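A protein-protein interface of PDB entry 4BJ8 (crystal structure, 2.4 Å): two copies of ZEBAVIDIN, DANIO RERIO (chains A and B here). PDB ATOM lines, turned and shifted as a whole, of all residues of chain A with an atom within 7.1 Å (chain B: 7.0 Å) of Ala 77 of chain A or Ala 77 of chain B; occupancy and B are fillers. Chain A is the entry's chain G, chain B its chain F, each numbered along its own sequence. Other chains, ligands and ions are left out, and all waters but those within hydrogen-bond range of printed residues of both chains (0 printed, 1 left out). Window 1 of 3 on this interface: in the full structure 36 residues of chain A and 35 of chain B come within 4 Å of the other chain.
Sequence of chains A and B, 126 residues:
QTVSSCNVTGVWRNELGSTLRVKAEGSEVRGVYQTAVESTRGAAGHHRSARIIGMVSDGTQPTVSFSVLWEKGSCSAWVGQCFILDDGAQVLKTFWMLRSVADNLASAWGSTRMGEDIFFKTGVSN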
ATOM      1  N   SER A  65     -21.791   6.946   5.051  1.00  0.00           N
ATOM      2  CA  SER A  65     -21.759   6.974   3.607  1.00  0.00           C
ATOM      3  C   SER A  65     -23.190   7.045   3.090  1.00  0.00           C
ATOM      4  O   SER A  65     -24.014   6.252   3.498  1.00  0.00           O
ATOM      5  CB  SER A  65     -21.092   5.704   3.069  1.00  0.00           C
ATOM      6  OG  SER A  65     -20.796   5.802   1.652  1.00  0.00           O
ATOM      7  N   PHE A  66     -23.507   7.989   2.208  1.00  0.00           N
ATOM      8  CA  PHE A  66     -24.843   8.014   1.620  1.00  0.00           C
ATOM      9  C   PHE A  66     -24.938   8.579   0.204  1.00  0.00           C
ATOM     10  O   PHE A  66     -24.042   9.256  -0.268  1.00  0.00           O
ATOM     11  CB  PHE A  66     -25.831   8.680   2.564  1.00  0.00           C
ATOM     12  CG  PHE A  66     -25.452  10.052   2.991  1.00  0.00           C
ATOM     13  CD1 PHE A  66     -24.658  10.243   4.085  1.00  0.00           C
ATOM     14  CD2 PHE A  66     -25.936  11.151   2.317  1.00  0.00           C
ATOM     15  CE1 PHE A  66     -24.327  11.494   4.509  1.00  0.00           C
ATOM     16  CE2 PHE A  66     -25.593  12.416   2.720  1.00  0.00           C
ATOM     17  CZ  PHE A  66     -24.782  12.586   3.823  1.00  0.00           C
ATOM     18  N   SER A  67     -26.030   8.239  -0.469  1.00  0.00           N
ATOM     19  CA  SER A  67     -26.175   8.454  -1.902  1.00  0.00           C
ATOM     20  C   SER A  67     -27.528   8.999  -2.202  1.00  0.00           C
ATOM     21  O   SER A  67     -28.494   8.682  -1.520  1.00  0.00           O
ATOM     22  CB  SER A  67     -26.116   7.149  -2.654  1.00  0.00           C
ATOM     23  OG  SER A  67     -24.897   6.518  -2.432  1.00  0.00           O
ATOM     24  N   VAL A  68     -27.595   9.747  -3.287  1.00  0.00           N
ATOM     25  CA  VAL A  68     -28.797  10.471  -3.668  1.00  0.00           C
ATOM     26  C   VAL A  68     -28.859  10.473  -5.200  1.00  0.00           C
ATOM     27  O   VAL A  68     -27.897  10.863  -5.870  1.00  0.00           O
ATOM     28  CB  VAL A  68     -28.741  11.901  -3.067  1.00  0.00           C
ATOM     29  CG1 VAL A  68     -29.853  12.803  -3.573  1.00  0.00           C
ATOM     30  CG2 VAL A  68     -28.781  11.829  -1.545  1.00  0.00           C
ATOM     31  N   TRP A  70     -30.795  12.247  -8.115  1.00  0.00           N
ATOM     32  CA  TRP A  70     -31.643  13.405  -8.349  1.00  0.00           C
ATOM     33  C   TRP A  70     -32.632  13.103  -9.484  1.00  0.00           C
ATOM     34  O   TRP A  70     -32.478  12.092 -10.175  1.00  0.00           O
ATOM     35  CB  TRP A  70     -30.793  14.638  -8.645  1.00  0.00           C
ATOM     36  CG  TRP A  70     -29.766  14.909  -7.582  1.00  0.00           C
ATOM     37  CD1 TRP A  70     -28.416  14.623  -7.631  1.00  0.00           C
ATOM     38  CD2 TRP A  70     -30.004  15.512  -6.322  1.00  0.00           C
ATOM     39  NE1 TRP A  70     -27.822  15.035  -6.482  1.00  0.00           N
ATOM     40  CE2 TRP A  70     -28.768  15.586  -5.660  1.00  0.00           C
ATOM     41  CE3 TRP A  70     -31.142  16.024  -5.695  1.00  0.00           C
ATOM     42  CZ2 TRP A  70     -28.636  16.119  -4.393  1.00  0.00           C
ATOM     43  CZ3 TRP A  70     -31.008  16.577  -4.437  1.00  0.00           C
ATOM     44  CH2 TRP A  70     -29.763  16.607  -3.791  1.00  0.00           C
ATOM     45  N   CYS A  75     -26.245  12.035  -9.996  1.00  0.00           N
ATOM     46  CA  CYS A  75     -26.259  11.442  -8.652  1.00  0.00           C
ATOM     47  C   CYS A  75     -25.120  11.987  -7.811  1.00  0.00           C
ATOM     48  O   CYS A  75     -24.133  12.474  -8.321  1.00  0.00           O
ATOM     49  CB  CYS A  75     -26.202   9.912  -8.703  1.00  0.00           C
ATOM     50  SG  CYS A  75     -24.727   9.249  -9.512  1.00  0.00           S
ATOM     51  N   SER A  76     -25.316  11.936  -6.499  1.00  0.00           N
ATOM     52  CA  SER A  76     -24.349  12.438  -5.545  1.00  0.00           C
ATOM     53  C   SER A  76     -24.084  11.420  -4.460  1.00  0.00           C
ATOM     54  O   SER A  76     -24.979  10.674  -4.078  1.00  0.00           O
ATOM     55  CB  SER A  76     -24.885  13.682  -4.885  1.00  0.00           C
ATOM     56  OG  SER A  76     -24.914  14.717  -5.809  1.00  0.00           O
ATOM     57  N   ALA A  77     -22.863  11.416  -3.941  1.00  0.00           N
ATOM     58  CA  ALA A  77     -22.523  10.578  -2.778  1.00  0.00           C
ATOM     59  C   ALA A  77     -21.665  11.363  -1.802  1.00  0.00           C
ATOM     60  O   ALA A  77     -20.842  12.167  -2.239  1.00  0.00           O
ATOM     61  CB  ALA A  77     -21.798   9.321  -3.228  1.00  0.00           C
ATOM     62  N   TRP A  78     -21.872  11.139  -0.495  1.00  0.00           N
ATOM     63  CA  TRP A  78     -21.055  11.757   0.560  1.00  0.00           C
ATOM     64  C   TRP A  78     -20.444  10.682   1.430  1.00  0.00           C
ATOM     65  O   TRP A  78     -21.113   9.703   1.756  1.00  0.00           O
ATOM     66  CB  TRP A  78     -21.881  12.577   1.525  1.00  0.00           C
ATOM     67  CG  TRP A  78     -22.490  13.848   1.037  1.00  0.00           C
ATOM     68  CD1 TRP A  78     -22.126  15.102   1.389  1.00  0.00           C
ATOM     69  CD2 TRP A  78     -23.607  13.978   0.156  1.00  0.00           C
ATOM     70  NE1 TRP A  78     -22.943  16.010   0.784  1.00  0.00           N
ATOM     71  CE2 TRP A  78     -23.859  15.341   0.012  1.00  0.00           C
ATOM     72  CE3 TRP A  78     -24.423  13.063  -0.517  1.00  0.00           C
ATOM     73  CZ2 TRP A  78     -24.894  15.829  -0.787  1.00  0.00           C
ATOM     74  CZ3 TRP A  78     -25.445  13.544  -1.310  1.00  0.00           C
ATOM     75  CH2 TRP A  78     -25.666  14.913  -1.441  1.00  0.00           C
ATOM     76  N   VAL A  79     -19.205  10.892   1.859  1.00  0.00           N
ATOM     77  CA  VAL A  79     -18.603  10.066   2.904  1.00  0.00           C
ATOM     78  C   VAL A  79     -18.150  10.965   4.058  1.00  0.00           C
ATOM     79  O   VAL A  79     -17.814  12.142   3.856  1.00  0.00           O
ATOM     80  CB  VAL A  79     -17.414   9.228   2.410  1.00  0.00           C
ATOM     81  CG1 VAL A  79     -17.867   8.220   1.365  1.00  0.00           C
ATOM     82  CG2 VAL A  79     -16.286  10.114   1.910  1.00  0.00           C
ATOM     83  N   PHE A  95     -17.177  14.741   2.624  1.00  0.00           N
ATOM     84  CA  PHE A  95     -16.847  15.134   1.247  1.00  0.00           C
ATOM     85  C   PHE A  95     -17.789  14.494   0.292  1.00  0.00           C
ATOM     86  O   PHE A  95     -18.204  13.337   0.504  1.00  0.00           O
ATOM     87  CB  PHE A  95     -15.432  14.703   0.847  1.00  0.00           C
ATOM     88  CG  PHE A  95     -14.410  15.582   1.387  1.00  0.00           C
ATOM     89  CD1 PHE A  95     -14.020  15.445   2.733  1.00  0.00           C
ATOM     90  CD2 PHE A  95     -13.905  16.596   0.622  1.00  0.00           C
ATOM     91  CE1 PHE A  95     -13.078  16.294   3.293  1.00  0.00           C
ATOM     92  CE2 PHE A  95     -12.974  17.474   1.151  1.00  0.00           C
ATOM     93  CZ  PHE A  95     -12.555  17.328   2.501  1.00  0.00           C
ATOM     94  N   TRP A  96     -18.054  15.191  -0.808  1.00  0.00           N
ATOM     95  CA  TRP A  96     -19.034  14.717  -1.735  1.00  0.00           C
ATOM     96  C   TRP A  96     -18.541  14.671  -3.161  1.00  0.00           C
ATOM     97  O   TRP A  96     -17.549  15.316  -3.478  1.00  0.00           O
ATOM     98  CB  TRP A  96     -20.303  15.558  -1.624  1.00  0.00           C
ATOM     99  CG  TRP A  96     -20.153  17.001  -1.845  1.00  0.00           C
ATOM    100  CD1 TRP A  96     -20.138  17.957  -0.889  1.00  0.00           C
ATOM    101  CD2 TRP A  96     -20.077  17.688  -3.103  1.00  0.00           C
ATOM    102  NE1 TRP A  96     -20.014  19.175  -1.448  1.00  0.00           N
ATOM    103  CE2 TRP A  96     -19.980  19.050  -2.813  1.00  0.00           C
ATOM    104  CE3 TRP A  96     -20.055  17.279  -4.438  1.00  0.00           C
ATOM    105  CZ2 TRP A  96     -19.847  20.024  -3.810  1.00  0.00           C
ATOM    106  CZ3 TRP A  96     -19.945  18.252  -5.450  1.00  0.00           C
ATOM    107  CH2 TRP A  96     -19.836  19.603  -5.122  1.00  0.00           C
ATOM    108  N   MET A  97     -19.267  13.916  -3.993  1.00  0.00           N
ATOM    109  CA  MET A  97     -19.046  13.814  -5.446  1.00  0.00           C
ATOM    110  C   MET A  97     -20.363  14.018  -6.140  1.00  0.00           C
ATOM    111  O   MET A  97     -21.360  13.433  -5.740  1.00  0.00           O
ATOM    112  CB  MET A  97     -18.544  12.427  -5.856  1.00  0.00           C
ATOM    113  CG  MET A  97     -17.105  12.136  -5.488  1.00  0.00           C
ATOM    114  SD  MET A  97     -16.492  10.517  -5.969  1.00  0.00           S
ATOM    115  CE  MET A  97     -17.649   9.409  -5.152  1.00  0.00           C
ATOM    116  N   LEU A  98     -20.381  14.864  -7.167  1.00  0.00           N
ATOM    117  CA  LEU A  98     -21.571  14.999  -8.003  1.00  0.00           C
ATOM    118  C   LEU A  98     -21.277  14.487  -9.387  1.00  0.00           C
ATOM    119  O   LEU A  98     -20.312  14.875  -9.995  1.00  0.00           O
ATOM    120  CB  LEU A  98     -22.068  16.429  -8.064  1.00  0.00           C
ATOM    121  CG  LEU A  98     -23.153  16.698  -9.106  1.00  0.00           C
ATOM    122  CD1 LEU A  98     -24.404  15.881  -8.836  1.00  0.00           C
ATOM    123  CD2 LEU A  98     -23.493  18.177  -9.095  1.00  0.00           C
ATOM    124  N   ARG A  99     -22.098  13.553  -9.836  1.00  0.00           N
ATOM    125  CA  ARG A  99     -21.927  12.932 -11.126  1.00  0.00           C
ATOM    126  C   ARG A  99     -23.011  13.484 -12.028  1.00  0.00           C
ATOM    127  O   ARG A  99     -24.204  13.284 -11.753  1.00  0.00           O
ATOM    128  CB  ARG A  99     -22.084  11.424 -11.009  1.00  0.00           C
ATOM    129  CG  ARG A  99     -21.842  10.681 -12.318  1.00  0.00           C
ATOM    130  CD  ARG A  99     -20.383  10.368 -12.456  1.00  0.00           C
ATOM    131  NE  ARG A  99     -19.953  10.099 -13.817  1.00  0.00           N
ATOM    132  CZ  ARG A  99     -18.770   9.568 -14.127  1.00  0.00           C
ATOM    133  NH1 ARG A  99     -17.911   9.259 -13.163  1.00  0.00           N
ATOM    134  NH2 ARG A  99     -18.454   9.337 -15.401  1.00  0.00           N
ATOM    135  N   GLY A 115     -16.660  18.383  -3.609  1.00  0.00           N
ATOM    136  CA  GLY A 115     -16.580  19.413  -2.573  1.00  0.00           C
ATOM    137  C   GLY A 115     -16.576  18.880  -1.133  1.00  0.00           C
ATOM    138  O   GLY A 115     -16.655  17.667  -0.908  1.00  0.00           O
ATOM    139  N   SER B  65     -25.032   5.208  -7.830  1.00  0.00           N
ATOM    140  CA  SER B  65     -24.378   5.723  -6.641  1.00  0.00           C
ATOM    141  C   SER B  65     -24.499   4.692  -5.536  1.00  0.00           C
ATOM    142  O   SER B  65     -25.618   4.413  -5.058  1.00  0.00           O
ATOM    143  CB  SER B  65     -25.010   7.046  -6.195  1.00  0.00           C
ATOM    144  OG  SER B  65     -24.322   7.576  -5.071  1.00  0.00           O
ATOM    145  N   PHE B  66     -23.371   4.119  -5.125  1.00  0.00           N
ATOM    146  CA  PHE B  66     -23.410   3.164  -4.010  1.00  0.00           C
ATOM    147  C   PHE B  66     -22.347   3.394  -2.927  1.00  0.00           C
ATOM    148  O   PHE B  66     -21.293   4.031  -3.182  1.00  0.00           O
ATOM    149  CB  PHE B  66     -23.382   1.730  -4.502  1.00  0.00           C
ATOM    150  CG  PHE B  66     -22.176   1.390  -5.290  1.00  0.00           C
ATOM    151  CD1 PHE B  66     -22.116   1.665  -6.640  1.00  0.00           C
ATOM    152  CD2 PHE B  66     -21.101   0.750  -4.692  1.00  0.00           C
ATOM    153  CE1 PHE B  66     -20.986   1.362  -7.373  1.00  0.00           C
ATOM    154  CE2 PHE B  66     -19.959   0.428  -5.428  1.00  0.00           C
ATOM    155  CZ  PHE B  66     -19.904   0.737  -6.774  1.00  0.00           C
ATOM    156  N   SER B  67     -22.670   2.871  -1.734  1.00  0.00           N
ATOM    157  CA  SER B  67     -21.825   2.937  -0.533  1.00  0.00           C
ATOM    158  C   SER B  67     -21.511   1.548  -0.044  1.00  0.00           C
ATOM    159  O   SER B  67     -22.302   0.621  -0.232  1.00  0.00           O
ATOM    160  CB  SER B  67     -22.563   3.584   0.662  1.00  0.00           C
ATOM    161  OG  SER B  67     -23.096   4.852   0.388  1.00  0.00           O
ATOM    162  N   VAL B  68     -20.409   1.467   0.678  1.00  0.00           N
ATOM    163  CA  VAL B  68     -20.019   0.300   1.434  1.00  0.00           C
ATOM    164  C   VAL B  68     -19.438   0.739   2.791  1.00  0.00           C
ATOM    165  O   VAL B  68     -18.612   1.661   2.861  1.00  0.00           O
ATOM    166  CB  VAL B  68     -18.893  -0.444   0.708  1.00  0.00           C
ATOM    167  CG1 VAL B  68     -18.353  -1.574   1.571  1.00  0.00           C
ATOM    168  CG2 VAL B  68     -19.389  -0.963  -0.618  1.00  0.00           C
ATOM    169  N   TRP B  70     -17.048  -0.692   5.673  1.00  0.00           N
ATOM    170  CA  TRP B  70     -16.058  -1.730   5.871  1.00  0.00           C
ATOM    171  C   TRP B  70     -15.979  -2.175   7.324  1.00  0.00           C
ATOM    172  O   TRP B  70     -16.447  -1.462   8.224  1.00  0.00           O
ATOM    173  CB  TRP B  70     -14.698  -1.237   5.405  1.00  0.00           C
ATOM    174  CG  TRP B  70     -14.670  -0.892   3.926  1.00  0.00           C
ATOM    175  CD1 TRP B  70     -14.571   0.340   3.390  1.00  0.00           C
ATOM    176  CD2 TRP B  70     -14.759  -1.799   2.828  1.00  0.00           C
ATOM    177  NE1 TRP B  70     -14.550   0.270   2.022  1.00  0.00           N
ATOM    178  CE2 TRP B  70     -14.684  -1.036   1.649  1.00  0.00           C
ATOM    179  CE3 TRP B  70     -14.860  -3.181   2.723  1.00  0.00           C
ATOM    180  CZ2 TRP B  70     -14.734  -1.611   0.375  1.00  0.00           C
ATOM    181  CZ3 TRP B  70     -14.893  -3.754   1.456  1.00  0.00           C
ATOM    182  CH2 TRP B  70     -14.833  -2.966   0.301  1.00  0.00           C
ATOM    183  N   CYS B  75     -15.298   3.728   5.267  1.00  0.00           N
ATOM    184  CA  CYS B  75     -16.359   3.571   4.275  1.00  0.00           C
ATOM    185  C   CYS B  75     -15.961   4.148   2.932  1.00  0.00           C
ATOM    186  O   CYS B  75     -15.097   5.023   2.836  1.00  0.00           O
ATOM    187  CB  CYS B  75     -17.633   4.238   4.744  1.00  0.00           C
ATOM    188  SG  CYS B  75     -17.399   5.992   5.004  1.00  0.00           S
ATOM    189  N   SER B  76     -16.601   3.640   1.894  1.00  0.00           N
ATOM    190  CA  SER B  76     -16.324   4.036   0.527  1.00  0.00           C
ATOM    191  C   SER B  76     -17.641   4.350  -0.207  1.00  0.00           C
ATOM    192  O   SER B  76     -18.667   3.739   0.078  1.00  0.00           O
ATOM    193  CB  SER B  76     -15.551   2.910  -0.163  1.00  0.00           C
ATOM    194  OG  SER B  76     -14.227   2.805   0.372  1.00  0.00           O
ATOM    195  N   ALA B  77     -17.600   5.315  -1.133  1.00  0.00           N
ATOM    196  CA  ALA B  77     -18.730   5.615  -2.013  1.00  0.00           C
ATOM    197  C   ALA B  77     -18.260   5.737  -3.450  1.00  0.00           C
ATOM    198  O   ALA B  77     -17.181   6.219  -3.718  1.00  0.00           O
ATOM    199  CB  ALA B  77     -19.423   6.905  -1.588  1.00  0.00           C
ATOM    200  N   TRP B  78     -19.097   5.303  -4.366  1.00  0.00           N
ATOM    201  CA  TRP B  78     -18.806   5.382  -5.760  1.00  0.00           C
ATOM    202  C   TRP B  78     -19.943   6.132  -6.389  1.00  0.00           C
ATOM    203  O   TRP B  78     -21.095   5.956  -5.992  1.00  0.00           O
ATOM    204  CB  TRP B  78     -18.784   3.992  -6.385  1.00  0.00           C
ATOM    205  CG  TRP B  78     -17.565   3.121  -6.098  1.00  0.00           C
ATOM    206  CD1 TRP B  78     -16.547   2.850  -6.947  1.00  0.00           C
ATOM    207  CD2 TRP B  78     -17.284   2.391  -4.883  1.00  0.00           C
ATOM    208  NE1 TRP B  78     -15.617   2.040  -6.333  1.00  0.00           N
ATOM    209  CE2 TRP B  78     -16.047   1.733  -5.071  1.00  0.00           C
ATOM    210  CE3 TRP B  78     -17.944   2.261  -3.644  1.00  0.00           C
ATOM    211  CZ2 TRP B  78     -15.462   0.915  -4.082  1.00  0.00           C
ATOM    212  CZ3 TRP B  78     -17.358   1.432  -2.646  1.00  0.00           C
ATOM    213  CH2 TRP B  78     -16.138   0.775  -2.879  1.00  0.00           C
ATOM    214  N   VAL B  79     -19.624   6.964  -7.376  1.00  0.00           N
ATOM    215  CA  VAL B  79     -20.617   7.500  -8.292  1.00  0.00           C
ATOM    216  C   VAL B  79     -20.168   7.126  -9.685  1.00  0.00           C
ATOM    217  O   VAL B  79     -18.962   7.043  -9.960  1.00  0.00           O
ATOM    218  CB  VAL B  79     -20.808   9.034  -8.176  1.00  0.00           C
ATOM    219  CG1 VAL B  79     -21.311   9.396  -6.793  1.00  0.00           C
ATOM    220  CG2 VAL B  79     -19.541   9.809  -8.497  1.00  0.00           C
ATOM    221  N   PHE B  95     -15.876   7.086 -10.029  1.00  0.00           N
ATOM    222  CA  PHE B  95     -14.890   7.669  -9.146  1.00  0.00           C
ATOM    223  C   PHE B  95     -15.353   7.365  -7.741  1.00  0.00           C
ATOM    224  O   PHE B  95     -16.538   7.228  -7.482  1.00  0.00           O
ATOM    225  CB  PHE B  95     -14.680   9.175  -9.392  1.00  0.00           C
ATOM    226  CG  PHE B  95     -13.789   9.460 -10.580  1.00  0.00           C
ATOM    227  CD1 PHE B  95     -12.416   9.513 -10.444  1.00  0.00           C
ATOM    228  CD2 PHE B  95     -14.340   9.644 -11.867  1.00  0.00           C
ATOM    229  CE1 PHE B  95     -11.594   9.749 -11.558  1.00  0.00           C
ATOM    230  CE2 PHE B  95     -13.528   9.889 -12.986  1.00  0.00           C
ATOM    231  CZ  PHE B  95     -12.151   9.935 -12.836  1.00  0.00           C
ATOM    232  N   TRP B  96     -14.395   7.201  -6.848  1.00  0.00           N
ATOM    233  CA  TRP B  96     -14.695   6.840  -5.461  1.00  0.00           C
ATOM    234  C   TRP B  96     -14.014   7.719  -4.408  1.00  0.00           C
ATOM    235  O   TRP B  96     -13.056   8.469  -4.670  1.00  0.00           O
ATOM    236  CB  TRP B  96     -14.339   5.383  -5.220  1.00  0.00           C
ATOM    237  CG  TRP B  96     -12.974   4.944  -5.671  1.00  0.00           C
ATOM    238  CD1 TRP B  96     -12.658   4.305  -6.823  1.00  0.00           C
ATOM    239  CD2 TRP B  96     -11.776   5.065  -4.935  1.00  0.00           C
ATOM    240  NE1 TRP B  96     -11.308   4.051  -6.873  1.00  0.00           N
ATOM    241  CE2 TRP B  96     -10.747   4.496  -5.710  1.00  0.00           C
ATOM    242  CE3 TRP B  96     -11.463   5.617  -3.689  1.00  0.00           C
ATOM    243  CZ2 TRP B  96      -9.434   4.446  -5.279  1.00  0.00           C
ATOM    244  CZ3 TRP B  96     -10.161   5.576  -3.260  1.00  0.00           C
ATOM    245  CH2 TRP B  96      -9.151   4.995  -4.051  1.00  0.00           C
ATOM    246  N   MET B  97     -14.562   7.640  -3.217  1.00  0.00           N
ATOM    247  CA  MET B  97     -13.912   8.204  -2.068  1.00  0.00           C
ATOM    248  C   MET B  97     -13.826   7.132  -1.017  1.00  0.00           C
ATOM    249  O   MET B  97     -14.723   6.331  -0.887  1.00  0.00           O
ATOM    250  CB  MET B  97     -14.725   9.367  -1.532  1.00  0.00           C
ATOM    251  CG  MET B  97     -14.913  10.482  -2.529  1.00  0.00           C
ATOM    252  SD  MET B  97     -15.903  11.783  -1.776  1.00  0.00           S
ATOM    253  CE  MET B  97     -17.525  11.021  -1.744  1.00  0.00           C
ATOM    254  N   LEU B  98     -12.736   7.133  -0.271  1.00  0.00           N
ATOM    255  CA  LEU B  98     -12.570   6.255   0.886  1.00  0.00           C
ATOM    256  C   LEU B  98     -12.290   7.111   2.131  1.00  0.00           C
ATOM    257  O   LEU B  98     -11.237   7.752   2.223  1.00  0.00           O
ATOM    258  CB  LEU B  98     -11.398   5.305   0.627  1.00  0.00           C
ATOM    259  CG  LEU B  98     -10.922   4.396   1.754  1.00  0.00           C
ATOM    260  CD1 LEU B  98     -12.002   3.497   2.352  1.00  0.00           C
ATOM    261  CD2 LEU B  98      -9.788   3.569   1.160  1.00  0.00           C
ATOM    262  N   ARG B  99     -13.230   7.138   3.074  1.00  0.00           N
ATOM    263  CA  ARG B  99     -12.967   7.822   4.335  1.00  0.00           C
ATOM    264  C   ARG B  99     -12.463   6.823   5.378  1.00  0.00           C
ATOM    265  O   ARG B  99     -13.081   5.786   5.570  1.00  0.00           O
ATOM    266  CB  ARG B  99     -14.191   8.595   4.860  1.00  0.00           C
ATOM    267  CG  ARG B  99     -13.893   9.437   6.103  1.00  0.00           C
ATOM    268  CD  ARG B  99     -14.989  10.420   6.417  1.00  0.00           C
ATOM    269  NE  ARG B  99     -14.666  11.801   6.006  1.00  0.00           N
ATOM    270  CZ  ARG B  99     -14.012  12.701   6.741  1.00  0.00           C
ATOM    271  NH1 ARG B  99     -13.596  12.453   7.957  1.00  0.00           N
ATOM    272  NH2 ARG B  99     -13.771  13.886   6.244  1.00  0.00           N
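Of the 15 printed residues of chain B, 10 touch a printed residue of chain A.
Printed residues of chain B that touch a printed residue of chain A: Ser 65, Phe 66, Ser 67, Ser 76, Ala 77, Val 79, Phe 95, Trp 96, Met 97 and Arg 99.
Hydrophobic or aromatic side chains of chain A that line the printed part of chain B: Ala 77, Val 79, Phe 95 and Met 97.
Among the printed residues, 26 pairs touch across the chains.
Among the printed residues, no Asp or Glu carboxylate lies within 4 Å of a Lys or Arg side-chain nitrogen of the other chain.
O of Phe 66 of chain A lies within hydrogen-bond range of N of Trp 78 of chain A (2.9 Å).
N of Val 68 of chain B lies within hydrogen-bond range of O of Ser 76 of chain B (2.9 Å).
The backbone NH (N) of Met 97 of chain A sits at hydrogen-bond distance from the backbone carbonyl oxygen (O) of Ala 77 of chain A, 2.9 Å away.
The indole nitrogen (NE1) of Trp 70 of chain B is in hydrogen-bond range of the side-chain hydroxyl (OG) of Ser 76 of chain B, 3.0 Å away.
O of Cys 75 of chain B is in hydrogen-bond range of N of Arg 99 of chain B (2.8 Å).
The backbone carbonyl oxygen (O) of Cys 75 of chain A is in hydrogen-bond range of the backbone NH (N) of Arg 99 of chain A, at 2.8 Å.
Printed residues of chain B within 4 Å of Cys 75 of chain A: Ser 65 (3.99 Å).
Printed residues of chain B within 4 Å of Ser 76 of chain A: Ser 65.
Of the printed residues of chain B, Ala 77 of chain A touches Ser 65, Ala 77, Val 79 and Met 97.
Trp 78 of chain A touches none of the printed residues of chain B.
Printed residues of chain B within 4 Å of Met 97 of chain A: Ala 77, Val 79, Phe 95, Trp 96 and Met 97.
Ala 77 of chain B touches just these residues of chain A: Ser 65, Ala 77, Val 79 and Met 97.
Printed residues of chain A within 4 Å of Trp 96 of chain B: Met 97.
Of the printed residues of chain A, Met 97 of chain B touches Ala 77, Val 79, Phe 95, Trp 96 and Met 97.
Leu 98 of chain B touches none of the printed residues of chain A.
The nearest residue of chain A that does not touch Ala 77 of chain B is Trp 78 of chain A (4.7 Å).
The nearest printed residue of chain B that does not touch Cys 75 of chain A is Val 79 of chain B (4.1 Å).
Ser 65 of chain A touches Ser 76 of chain B, and with the chains exchanged Ser 76 of chain A touches Ser 65 of chain B.
Ser 65 of chain A touches Ala 77 of chain B, and with the chains exchanged Ala 77 of chain A touches Ser 65 of chain B.
Ser 67 of chain B touches its own counterpart, Ser 67 of chain A.
Phe 95 of chain A touches Met 97 of chain B, and with the chains exchanged Met 97 of chain A touches Phe 95 of chain B.
Of the 26 pairs that touch across the chains among the printed residues, 25 have their exchanged pair printed and touching as well.
Phe 66 of chain A touches Ser 67 of chain B (N to OG, 3.6 Å).
Ser 67 of chain A touches Ser 67 of chain B (OG to OG, 3.7 Å).
Ala 77 of chain A touches Ser 65 of chain B (CB to OG, 3.6 Å).
CB of Ala 77 of chain A touches CB of Ala 77 of chain B (3.8 Å).
O of Ala 77 of chain A touches CE of Met 97 of chain B, at 3.5 Å.
CG2 of Val 79 of chain A touches CB of Met 97 of chain B, 3.9 Å away.
Val 79 of chain A touches Arg 99 of chain B (O to NE, 3.8 Å).
NH2 of Arg 99 of chain B touches CD1 of Phe 95 of chain A, 3.8 Å away.
Trp 96 of chain A touches Met 97 of chain B (CA to CE, 3.99 Å).
CE of Met 97 of chain A touches O of Ala 77 of chain B, at 3.5 Å.
The side-chain hydroxyl (OG) of Ser 65 of chain A lies within hydrogen-bond range of the side-chain hydroxyl (OG) of Ser 67 of chain B, 2.8 Å away.
OG of Ser 67 of chain A lies within hydrogen-bond range of OG of Ser 65 of chain B (2.9 Å).
The backbone carbonyl oxygen of Ser 76 of chain A lies within hydrogen-bond range of the side-chain hydroxyl of Ser 65 of chain B.
The side-chain hydroxyl of Ser 65 of chain A sits at hydrogen-bond distance from the backbone carbonyl oxygen of Ser 76 of chain B (3.4 Å).
SD of Met 97 of chain B lies close to O of Phe 95 of chain A, 3.6 Å away.
The side-chain sulfur (SD) of Met 97 of chain A lies close to the backbone carbonyl oxygen (O) of Phe 95 of chain B.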
